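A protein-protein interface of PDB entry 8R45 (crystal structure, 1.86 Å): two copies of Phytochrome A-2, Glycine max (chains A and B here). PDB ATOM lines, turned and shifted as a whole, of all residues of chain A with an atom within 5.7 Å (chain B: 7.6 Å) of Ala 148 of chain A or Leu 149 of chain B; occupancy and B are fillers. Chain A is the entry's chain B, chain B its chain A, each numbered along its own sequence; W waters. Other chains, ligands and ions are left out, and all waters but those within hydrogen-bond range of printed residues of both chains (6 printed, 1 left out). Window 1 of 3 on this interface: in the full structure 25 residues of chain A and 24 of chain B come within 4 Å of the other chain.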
ATOM      1  N   ASN A 105       9.992   8.929  14.181  1.00  0.00           N
ATOM      2  CA  ASN A 105      11.428   8.810  13.937  1.00  0.00           C
ATOM      3  C   ASN A 105      11.894   7.401  14.320  1.00  0.00           C
ATOM      4  O   ASN A 105      11.194   6.691  15.045  1.00  0.00           O
ATOM      5  CB  ASN A 105      12.177   9.845  14.776  1.00  0.00           C
ATOM      6  CG  ASN A 105      12.135  11.235  14.169  1.00  0.00           C
ATOM      7  OD1 ASN A 105      12.423  11.402  12.987  1.00  0.00           O
ATOM      8  ND2 ASN A 105      11.821  12.240  14.985  1.00  0.00           N
ATOM      9  N   PRO A 106      13.080   6.948  13.852  1.00  0.00           N
ATOM     10  CA  PRO A 106      13.874   7.664  12.841  1.00  0.00           C
ATOM     11  C   PRO A 106      13.477   7.249  11.430  1.00  0.00           C
ATOM     12  O   PRO A 106      12.852   6.203  11.312  1.00  0.00           O
ATOM     13  CB  PRO A 106      15.278   7.136  13.163  1.00  0.00           C
ATOM     14  CG  PRO A 106      15.017   5.651  13.501  1.00  0.00           C
ATOM     15  CD  PRO A 106      13.647   5.616  14.173  1.00  0.00           C
ATOM     16  N   MET A 143      18.405  -5.442  10.107  1.00  0.00           N
ATOM     17  CA  MET A 143      17.880  -5.682  11.431  1.00  0.00           C
ATOM     18  C   MET A 143      17.236  -4.417  12.011  1.00  0.00           C
ATOM     19  O   MET A 143      17.043  -4.340  13.226  1.00  0.00           O
ATOM     20  CB  MET A 143      19.008  -6.170  12.356  1.00  0.00           C
ATOM     21  CG  MET A 143      19.741  -7.387  11.832  1.00  0.00           C
ATOM     22  SD  MET A 143      18.596  -8.757  11.446  1.00  0.00           S
ATOM     23  CE  MET A 143      18.144  -9.253  13.093  1.00  0.00           C
ATOM     24  N   THR A 144      16.919  -3.431  11.161  1.00  0.00           N
ATOM     25  CA  THR A 144      16.443  -2.136  11.608  1.00  0.00           C
ATOM     26  C   THR A 144      15.165  -2.238  12.459  1.00  0.00           C
ATOM     27  O   THR A 144      15.082  -1.728  13.581  1.00  0.00           O
ATOM     28  CB  THR A 144      16.237  -1.229  10.383  1.00  0.00           C
ATOM     29  OG1 THR A 144      15.914   0.023  10.937  1.00  0.00           O
ATOM     30  CG2 THR A 144      15.125  -1.592   9.439  1.00  0.00           C
ATOM     31  N   ALA A 145      14.173  -2.980  11.968  1.00  0.00           N
ATOM     32  CA  ALA A 145      12.932  -3.143  12.725  1.00  0.00           C
ATOM     33  C   ALA A 145      13.154  -4.084  13.898  1.00  0.00           C
ATOM     34  O   ALA A 145      12.656  -3.858  15.012  1.00  0.00           O
ATOM     35  CB  ALA A 145      11.853  -3.630  11.772  1.00  0.00           C
ATOM     36  N   ALA A 146      13.920  -5.165  13.662  1.00  0.00           N
ATOM     37  CA  ALA A 146      14.192  -6.134  14.691  1.00  0.00           C
ATOM     38  C   ALA A 146      14.856  -5.478  15.873  1.00  0.00           C
ATOM     39  O   ALA A 146      14.500  -5.757  17.004  1.00  0.00           O
ATOM     40  CB  ALA A 146      15.034  -7.293  14.166  1.00  0.00           C
ATOM     41  N   GLY A 147      15.858  -4.626  15.644  1.00  0.00           N
ATOM     42  CA  GLY A 147      16.546  -4.018  16.757  1.00  0.00           C
ATOM     43  C   GLY A 147      15.717  -2.948  17.474  1.00  0.00           C
ATOM     44  O   GLY A 147      15.829  -2.808  18.692  1.00  0.00           O
ATOM     45  N   ALA A 148      14.858  -2.257  16.725  1.00  0.00           N
ATOM     46  CA  ALA A 148      13.939  -1.306  17.331  1.00  0.00           C
ATOM     47  C   ALA A 148      12.942  -2.020  18.255  1.00  0.00           C
ATOM     48  O   ALA A 148      12.751  -1.597  19.389  1.00  0.00           O
ATOM     49  CB  ALA A 148      13.280  -0.502  16.278  1.00  0.00           C
ATOM     50  N   LEU A 149      12.328  -3.119  17.796  1.00  0.00           N
ATOM     51  CA  LEU A 149      11.407  -3.885  18.632  1.00  0.00           C
ATOM     52  C   LEU A 149      12.106  -4.401  19.895  1.00  0.00           C
ATOM     53  O   LEU A 149      11.525  -4.384  20.974  1.00  0.00           O
ATOM     54  CB  LEU A 149      10.826  -5.043  17.819  1.00  0.00           C
ATOM     55  CG  LEU A 149       9.901  -4.636  16.672  1.00  0.00           C
ATOM     56  CD1 LEU A 149       9.583  -5.828  15.757  1.00  0.00           C
ATOM     57  CD2 LEU A 149       8.598  -4.025  17.214  1.00  0.00           C
ATOM     58  N   GLN A 150      13.328  -4.939  19.741  1.00  0.00           N
ATOM     59  CA  GLN A 150      14.035  -5.496  20.876  1.00  0.00           C
ATOM     60  C   GLN A 150      14.351  -4.406  21.888  1.00  0.00           C
ATOM     61  O   GLN A 150      14.245  -4.671  23.081  1.00  0.00           O
ATOM     62  CB  GLN A 150      15.311  -6.202  20.395  1.00  0.00           C
ATOM     63  CG  GLN A 150      16.151  -6.766  21.535  1.00  0.00           C
ATOM     64  CD  GLN A 150      15.541  -7.966  22.219  1.00  0.00           C
ATOM     65  OE1 GLN A 150      14.450  -8.458  21.921  1.00  0.00           O
ATOM     66  NE2 GLN A 150      16.272  -8.452  23.201  1.00  0.00           N
ATOM     67  N   SER A 151      14.780  -3.204  21.448  1.00  0.00           N
ATOM     68  CA  SER A 151      15.074  -2.142  22.391  1.00  0.00           C
ATOM     69  C   SER A 151      13.806  -1.760  23.169  1.00  0.00           C
ATOM     70  O   SER A 151      13.822  -1.596  24.405  1.00  0.00           O
ATOM     71  CB  SER A 151      15.700  -0.934  21.713  1.00  0.00           C
ATOM     72  OG  SER A 151      16.941  -1.238  21.084  1.00  0.00           O
ATOM     73  N   TYR A 152      12.686  -1.642  22.461  1.00  0.00           N
ATOM     74  CA  TYR A 152      11.456  -1.222  23.111  1.00  0.00           C
ATOM     75  C   TYR A 152      10.908  -2.346  23.978  1.00  0.00           C
ATOM     76  O   TYR A 152      10.410  -2.081  25.065  1.00  0.00           O
ATOM     77  CB  TYR A 152      10.406  -0.726  22.106  1.00  0.00           C
ATOM     78  CG  TYR A 152       9.700   0.523  22.568  1.00  0.00           C
ATOM     79  CD1 TYR A 152       8.811   0.509  23.633  1.00  0.00           C
ATOM     80  CD2 TYR A 152       9.994   1.746  22.014  1.00  0.00           C
ATOM     81  CE1 TYR A 152       8.205   1.664  24.088  1.00  0.00           C
ATOM     82  CE2 TYR A 152       9.388   2.910  22.450  1.00  0.00           C
ATOM     83  CZ  TYR A 152       8.475   2.875  23.493  1.00  0.00           C
ATOM     84  OH  TYR A 152       7.847   4.028  23.935  1.00  0.00           O
ATOM     85  N   LYS A 153      11.064  -3.607  23.560  1.00  0.00           N
ATOM     86  CA  LYS A 153      10.671  -4.738  24.395  1.00  0.00           C
ATOM     87  C   LYS A 153      11.465  -4.737  25.695  1.00  0.00           C
ATOM     88  O   LYS A 153      10.885  -4.946  26.754  1.00  0.00           O
ATOM     89  CB  LYS A 153      10.870  -6.066  23.657  1.00  0.00           C
ATOM     90  CG  LYS A 153      10.676  -7.333  24.470  1.00  0.00           C
ATOM     91  CD  LYS A 153      10.732  -8.568  23.598  1.00  0.00           C
ATOM     92  CE  LYS A 153      10.355  -9.849  24.311  1.00  0.00           C
ATOM     93  NZ  LYS A 153      10.616 -11.023  23.438  1.00  0.00           N
ATOM     94  N   PHE A 330      19.565   5.660  17.955  1.00  0.00           N
ATOM     95  CA  PHE A 330      18.373   6.400  18.258  1.00  0.00           C
ATOM     96  C   PHE A 330      17.258   5.501  18.808  1.00  0.00           C
ATOM     97  O   PHE A 330      16.606   5.869  19.799  1.00  0.00           O
ATOM     98  CB  PHE A 330      17.916   7.234  17.058  1.00  0.00           C
ATOM     99  CG  PHE A 330      16.607   7.904  17.354  1.00  0.00           C
ATOM    100  CD1 PHE A 330      16.549   9.064  18.110  1.00  0.00           C
ATOM    101  CD2 PHE A 330      15.409   7.316  16.965  1.00  0.00           C
ATOM    102  CE1 PHE A 330      15.323   9.636  18.429  1.00  0.00           C
ATOM    103  CE2 PHE A 330      14.190   7.864  17.341  1.00  0.00           C
ATOM    104  CZ  PHE A 330      14.153   9.031  18.064  1.00  0.00           C
ATOM    105  N   PRO A 331      16.960   4.314  18.233  1.00  0.00           N
ATOM    106  CA  PRO A 331      15.822   3.537  18.740  1.00  0.00           C
ATOM    107  C   PRO A 331      15.931   3.230  20.232  1.00  0.00           C
ATOM    108  O   PRO A 331      14.943   3.289  20.967  1.00  0.00           O
ATOM    109  CB  PRO A 331      15.838   2.293  17.816  1.00  0.00           C
ATOM    110  CG  PRO A 331      16.397   2.839  16.531  1.00  0.00           C
ATOM    111  CD  PRO A 331      17.537   3.725  17.025  1.00  0.00           C
ATOM    112  N   TYR A 334      15.163   6.362  22.161  1.00  0.00           N
ATOM    113  CA  TYR A 334      13.741   6.607  22.102  1.00  0.00           C
ATOM    114  C   TYR A 334      13.021   5.766  23.159  1.00  0.00           C
ATOM    115  O   TYR A 334      12.147   6.246  23.902  1.00  0.00           O
ATOM    116  CB  TYR A 334      13.267   6.354  20.669  1.00  0.00           C
ATOM    117  CG  TYR A 334      11.855   6.805  20.391  1.00  0.00           C
ATOM    118  CD1 TYR A 334      11.484   8.136  20.525  1.00  0.00           C
ATOM    119  CD2 TYR A 334      10.888   5.894  19.988  1.00  0.00           C
ATOM    120  CE1 TYR A 334      10.190   8.562  20.236  1.00  0.00           C
ATOM    121  CE2 TYR A 334       9.601   6.295  19.700  1.00  0.00           C
ATOM    122  CZ  TYR A 334       9.236   7.630  19.847  1.00  0.00           C
ATOM    123  OH  TYR A 334       7.966   8.042  19.498  1.00  0.00           O
ATOM    124  N   ALA A 335      13.378   4.493  23.218  1.00  0.00           N
ATOM    125  CA  ALA A 335      12.792   3.606  24.197  1.00  0.00           C
ATOM    126  C   ALA A 335      13.151   4.108  25.589  1.00  0.00           C
ATOM    127  O   ALA A 335      12.323   3.991  26.483  1.00  0.00           O
ATOM    128  CB  ALA A 335      13.254   2.194  23.996  1.00  0.00           C
ATOM    129  N   ASN B 105      13.203 -10.917  15.301  1.00  0.00           N
ATOM    130  CA  ASN B 105      12.408 -10.779  14.078  1.00  0.00           C
ATOM    131  C   ASN B 105      11.813  -9.384  14.031  1.00  0.00           C
ATOM    132  O   ASN B 105      11.679  -8.727  15.068  1.00  0.00           O
ATOM    133  CB  ASN B 105      11.278 -11.801  14.032  1.00  0.00           C
ATOM    134  CG  ASN B 105      11.774 -13.172  13.589  1.00  0.00           C
ATOM    135  OD1 ASN B 105      12.472 -13.290  12.578  1.00  0.00           O
ATOM    136  ND2 ASN B 105      11.405 -14.203  14.314  1.00  0.00           N
ATOM    137  N   MET B 143      10.591   3.843   6.587  1.00  0.00           N
ATOM    138  CA  MET B 143       9.868   4.034   7.826  1.00  0.00           C
ATOM    139  C   MET B 143       9.754   2.735   8.627  1.00  0.00           C
ATOM    140  O   MET B 143       8.986   2.671   9.582  1.00  0.00           O
ATOM    141  CB  MET B 143       8.452   4.580   7.580  1.00  0.00           C
ATOM    142  CG  MET B 143       8.444   5.873   6.812  1.00  0.00           C
ATOM    143  SD  MET B 143       9.499   7.159   7.530  1.00  0.00           S
ATOM    144  CE  MET B 143       8.652   7.476   9.067  1.00  0.00           C
ATOM    145  N   THR B 144      10.513   1.674   8.284  1.00  0.00           N
ATOM    146  CA  THR B 144      10.306   0.401   8.982  1.00  0.00           C
ATOM    147  C   THR B 144      10.627   0.492  10.473  1.00  0.00           C
ATOM    148  O   THR B 144       9.821   0.006  11.263  1.00  0.00           O
ATOM    149  CB  THR B 144      11.040  -0.799   8.343  1.00  0.00           C
ATOM    150  OG1 THR B 144      12.410  -0.486   8.254  1.00  0.00           O
ATOM    151  CG2 THR B 144      10.654  -1.063   6.918  1.00  0.00           C
ATOM    152  N   ALA B 145      11.793   1.023  10.864  1.00  0.00           N
ATOM    153  CA  ALA B 145      12.094   1.181  12.286  1.00  0.00           C
ATOM    154  C   ALA B 145      11.115   2.112  12.978  1.00  0.00           C
ATOM    155  O   ALA B 145      10.679   1.822  14.089  1.00  0.00           O
ATOM    156  CB  ALA B 145      13.526   1.661  12.513  1.00  0.00           C
ATOM    157  N   ALA B 146      10.770   3.226  12.324  1.00  0.00           N
ATOM    158  CA  ALA B 146       9.835   4.217  12.874  1.00  0.00           C
ATOM    159  C   ALA B 146       8.500   3.559  13.206  1.00  0.00           C
ATOM    160  O   ALA B 146       7.943   3.768  14.293  1.00  0.00           O
ATOM    161  CB  ALA B 146       9.656   5.381  11.895  1.00  0.00           C
ATOM    162  N   GLY B 147       8.005   2.729  12.271  1.00  0.00           N
ATOM    163  CA  GLY B 147       6.706   2.090  12.431  1.00  0.00           C
ATOM    164  C   GLY B 147       6.709   1.007  13.506  1.00  0.00           C
ATOM    165  O   GLY B 147       5.743   0.835  14.253  1.00  0.00           O
ATOM    166  N   ALA B 148       7.836   0.334  13.636  1.00  0.00           N
ATOM    167  CA  ALA B 148       8.011  -0.682  14.650  1.00  0.00           C
ATOM    168  C   ALA B 148       8.062  -0.038  16.033  1.00  0.00           C
ATOM    169  O   ALA B 148       7.412  -0.554  16.937  1.00  0.00           O
ATOM    170  CB  ALA B 148       9.266  -1.486  14.382  1.00  0.00           C
ATOM    171  N   LEU B 149       8.846   1.023  16.193  1.00  0.00           N
ATOM    172  CA  LEU B 149       8.848   1.761  17.454  1.00  0.00           C
ATOM    173  C   LEU B 149       7.449   2.267  17.800  1.00  0.00           C
ATOM    174  O   LEU B 149       7.065   2.153  18.949  1.00  0.00           O
ATOM    175  CB  LEU B 149       9.805   2.954  17.432  1.00  0.00           C
ATOM    176  CG  LEU B 149      11.273   2.560  17.278  1.00  0.00           C
ATOM    177  CD1 LEU B 149      12.105   3.754  16.917  1.00  0.00           C
ATOM    178  CD2 LEU B 149      11.799   1.875  18.526  1.00  0.00           C
ATOM    179  N   GLN B 150       6.729   2.875  16.846  1.00  0.00           N
ATOM    180  CA  GLN B 150       5.400   3.400  17.151  1.00  0.00           C
ATOM    181  C   GLN B 150       4.454   2.278  17.582  1.00  0.00           C
ATOM    182  O   GLN B 150       3.695   2.455  18.524  1.00  0.00           O
ATOM    183  CB  GLN B 150       4.905   4.200  15.945  1.00  0.00           C
ATOM    184  CG  GLN B 150       3.503   4.731  16.081  1.00  0.00           C
ATOM    185  CD  GLN B 150       3.415   5.871  17.062  1.00  0.00           C
ATOM    186  OE1 GLN B 150       4.379   6.291  17.707  1.00  0.00           O
ATOM    187  NE2 GLN B 150       2.207   6.364  17.236  1.00  0.00           N
ATOM    188  N   SER B 151       4.493   1.100  16.938  1.00  0.00           N
ATOM    189  CA  SER B 151       3.663  -0.024  17.342  1.00  0.00           C
ATOM    190  C   SER B 151       3.950  -0.422  18.782  1.00  0.00           C
ATOM    191  O   SER B 151       3.036  -0.685  19.558  1.00  0.00           O
ATOM    192  CB  SER B 151       3.828  -1.222  16.422  1.00  0.00           C
ATOM    193  OG  SER B 151       3.318  -0.905  15.126  1.00  0.00           O
ATOM    194  N   TYR B 152       5.235  -0.490  19.148  1.00  0.00           N
ATOM    195  CA  TYR B 152       5.544  -0.986  20.482  1.00  0.00           C
ATOM    196  C   TYR B 152       5.263   0.098  21.500  1.00  0.00           C
ATOM    197  O   TYR B 152       4.794  -0.198  22.586  1.00  0.00           O
ATOM    198  CB  TYR B 152       6.984  -1.476  20.576  1.00  0.00           C
ATOM    199  CG  TYR B 152       7.116  -2.735  21.389  1.00  0.00           C
ATOM    200  CD1 TYR B 152       6.958  -2.722  22.753  1.00  0.00           C
ATOM    201  CD2 TYR B 152       7.319  -3.965  20.786  1.00  0.00           C
ATOM    202  CE1 TYR B 152       7.065  -3.891  23.493  1.00  0.00           C
ATOM    203  CE2 TYR B 152       7.431  -5.136  21.513  1.00  0.00           C
ATOM    204  CZ  TYR B 152       7.276  -5.108  22.875  1.00  0.00           C
ATOM    205  OH  TYR B 152       7.335  -6.259  23.624  1.00  0.00           O
ATOM    206  N   LYS B 153       5.482   1.362  21.126  1.00  0.00           N
ATOM    207  CA  LYS B 153       5.141   2.473  22.000  1.00  0.00           C
ATOM    208  C   LYS B 153       3.662   2.467  22.353  1.00  0.00           C
ATOM    209  O   LYS B 153       3.292   2.609  23.531  1.00  0.00           O
ATOM    210  CB  LYS B 153       5.575   3.797  21.357  1.00  0.00           C
ATOM    211  CG  LYS B 153       5.192   5.050  22.150  1.00  0.00           C
ATOM    212  CD  LYS B 153       5.685   6.316  21.471  1.00  0.00           C
ATOM    213  CE  LYS B 153       5.117   7.580  22.077  1.00  0.00           C
ATOM    214  NZ  LYS B 153       5.814   8.773  21.544  1.00  0.00           N
ATOM    215  N   LEU B 154       2.798   2.330  21.333  1.00  0.00           N
ATOM    216  CA  LEU B 154       1.363   2.276  21.570  1.00  0.00           C
ATOM    217  C   LEU B 154       0.985   1.107  22.477  1.00  0.00           C
ATOM    218  O   LEU B 154       0.194   1.303  23.398  1.00  0.00           O
ATOM    219  CB  LEU B 154       0.608   2.203  20.242  1.00  0.00           C
ATOM    220  CG  LEU B 154       0.700   3.442  19.359  1.00  0.00           C
ATOM    221  CD1 LEU B 154       0.140   3.141  17.983  1.00  0.00           C
ATOM    222  CD2 LEU B 154      -0.022   4.632  20.005  1.00  0.00           C
ATOM    223  N   ALA B 155       1.608  -0.068  22.276  1.00  0.00           N
ATOM    224  CA  ALA B 155       1.355  -1.229  23.112  1.00  0.00           C
ATOM    225  C   ALA B 155       1.824  -0.991  24.538  1.00  0.00           C
ATOM    226  O   ALA B 155       1.172  -1.441  25.498  1.00  0.00           O
ATOM    227  CB  ALA B 155       2.030  -2.463  22.552  1.00  0.00           C
ATOM    228  N   ALA B 156       2.994  -0.357  24.655  1.00  0.00           N
ATOM    229  CA  ALA B 156       3.590  -0.094  25.966  1.00  0.00           C
ATOM    230  C   ALA B 156       2.703   0.844  26.780  1.00  0.00           C
ATOM    231  O   ALA B 156       2.544   0.625  27.992  1.00  0.00           O
ATOM    232  CB  ALA B 156       4.988   0.437  25.835  1.00  0.00           C
ATOM    233  N   PRO B 331       5.510  -6.266  13.028  1.00  0.00           N
ATOM    234  CA  PRO B 331       5.820  -5.531  14.259  1.00  0.00           C
ATOM    235  C   PRO B 331       4.644  -5.262  15.189  1.00  0.00           C
ATOM    236  O   PRO B 331       4.821  -5.312  16.403  1.00  0.00           O
ATOM    237  CB  PRO B 331       6.486  -4.244  13.754  1.00  0.00           C
ATOM    238  CG  PRO B 331       7.118  -4.695  12.444  1.00  0.00           C
ATOM    239  CD  PRO B 331       6.056  -5.597  11.835  1.00  0.00           C
ATOM    240  N   TYR B 334       3.769  -8.493  16.847  1.00  0.00           N
ATOM    241  CA  TYR B 334       4.783  -8.743  17.853  1.00  0.00           C
ATOM    242  C   TYR B 334       4.521  -7.919  19.120  1.00  0.00           C
ATOM    243  O   TYR B 334       4.635  -8.441  20.245  1.00  0.00           O
ATOM    244  CB  TYR B 334       6.180  -8.508  17.276  1.00  0.00           C
ATOM    245  CG  TYR B 334       7.314  -8.927  18.154  1.00  0.00           C
ATOM    246  CD1 TYR B 334       7.562 -10.274  18.381  1.00  0.00           C
ATOM    247  CD2 TYR B 334       8.175  -7.996  18.729  1.00  0.00           C
ATOM    248  CE1 TYR B 334       8.591 -10.694  19.206  1.00  0.00           C
ATOM    249  CE2 TYR B 334       9.256  -8.396  19.491  1.00  0.00           C
ATOM    250  CZ  TYR B 334       9.463  -9.755  19.731  1.00  0.00           C
ATOM    251  OH  TYR B 334      10.532 -10.258  20.465  1.00  0.00           O
ATOM    252  N   ALA B 335       4.248  -6.613  18.953  1.00  0.00           N
ATOM    253  CA  ALA B 335       3.862  -5.776  20.076  1.00  0.00           C
ATOM    254  C   ALA B 335       2.604  -6.330  20.753  1.00  0.00           C
ATOM    255  O   ALA B 335       2.524  -6.329  21.989  1.00  0.00           O
ATOM    256  CB  ALA B 335       3.649  -4.345  19.640  1.00  0.00           C
HETATM  257  O   HOH W   1      10.856 -13.342  21.202  1.00  0.00           O
HETATM  258  O   HOH W   2       6.979   6.305  17.971  1.00  0.00           O
HETATM  259  O   HOH W   3      14.263   1.560   9.290  1.00  0.00           O
HETATM  260  O   HOH W   4      13.072  -8.275  17.439  1.00  0.00           O
HETATM  261  O   HOH W   5       8.516   6.234  15.531  1.00  0.00           O
HETATM  262  O   HOH W   6      12.498  -8.398  20.129  1.00  0.00           O
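Water W2 bridges the side-chain hydroxyl (OH) of Tyr 334 of chain A (2.5 Å) and the side-chain amide oxygen (OE1) of Gln 150 of chain B (2.6 Å).
Water W6 lies within hydrogen-bond range of OE1 of Gln 150 of chain A (2.7 Å) and OH of Tyr 334 of chain B (2.7 Å).
Water W5 bridges the backbone carbonyl oxygen of Asn 105 of chain A (2.8 Å) and the backbone carbonyl oxygen of Ala 146 of chain B (2.8 Å).
Water W4 lies within hydrogen-bond range of the backbone carbonyl oxygen (O) of Asn 105 of chain B and the backbone carbonyl oxygen (O) of Ala 146 of chain A.
Water W3 lies within hydrogen-bond range of OG1 of Thr 144 of chain A (2.8 Å), OG1 of Thr 144 of chain B (2.9 Å) and N of Ala 145 of chain B (3.0 Å).
Water W1 bridges OH of Tyr 334 of chain B (3.2 Å) and NZ of Lys 153 of chain A (3.2 Å).
Of the 17 printed residues of chain A, 9 touch a printed residue of chain B.
Hydrophobic or aromatic side chains of chain A within 4 Å of the printed part of chain B: Pro 106, Ala 146, Ala 148, Leu 149, Tyr 152 and Tyr 334.
Hydrophobic or aromatic side chains of chain B that line the printed part of chain A: Ala 145, Ala 146, Ala 148, Leu 149, Tyr 152, Ala 156 and Tyr 334.
Among the printed residues, 20 pairs touch across the chains.
Among the printed residues, no Asp or Glu carboxylate lies within 4 Å of a Lys or Arg side-chain nitrogen of the other chain.
OH of Tyr 334 of chain A lies within hydrogen-bond range of NZ of Lys 153 of chain B, 3.1 Å away.
The side-chain hydroxyl (OH) of Tyr 334 of chain B is in hydrogen-bond range of the side-chain amino group (NZ) of Lys 153 of chain A, 3.1 Å away.
Asn 105 of chain A touches Ala 146 of chain B (O to CA, 3.6 Å).
Asn 105 of chain A touches Leu 149 of chain B (O to CD1, 3.6 Å).
Pro 106 of chain A touches Ala 146 of chain B.
Pro 106 of chain A touches Leu 149 of chain B.
Ala 145 of chain B touches Thr 144 of chain A (CB to OG1, 3.3 Å).
O of Asn 105 of chain B touches CA of Ala 146 of chain A (3.6 Å).
Ala 148 of chain A touches Leu 149 of chain B.
Leu 149 of chain A touches Asn 105 of chain B.
Leu 149 of chain A touches Ala 148 of chain B.
Leu 149 of chain B touches Tyr 334 of chain A.
Of chain B, only Leu 149 (3.6 Å) comes within 4 Å of Ala 148 of chain A.
No residue of chain B comes within 4 Å of Gly 147 of chain A.
Of the printed residues of chain A, Asn 105 of chain B touches Ala 146 (3.6 Å) and Leu 149 (3.6 Å).
Printed residues of chain A within 4 Å of Ala 145 of chain B: Thr 144 (3.3 Å).
Printed residues of chain B within 4 Å of Lys 153 of chain A: Tyr 152 (3.5 Å) and Tyr 334 (3.1 Å).
Printed residues of chain A within 4 Å of Thr 144 of chain B: Thr 144 (3.2 Å).
Ala 145 of chain A touches none of the printed residues of chain B.
Asn 105 of chain A touches Ala 146 of chain B, and with the chains exchanged Ala 146 of chain A touches Asn 105 of chain B.
Asn 105 of chain A touches Leu 149 of chain B, and with the chains exchanged Leu 149 of chain A touches Asn 105 of chain B.
Thr 144 of chain A touches Ala 145 of chain B, but with the chains exchanged Ala 145 of chain A does not touch Thr 144 of chain B (4.2 Å).
Tyr 152 of chain B touches its own counterpart, Tyr 152 of chain A.
15 positions are printed for both chains.
Of the 20 pairs that touch across the chains among the printed residues, 16 have their exchanged pair printed and touching as well.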
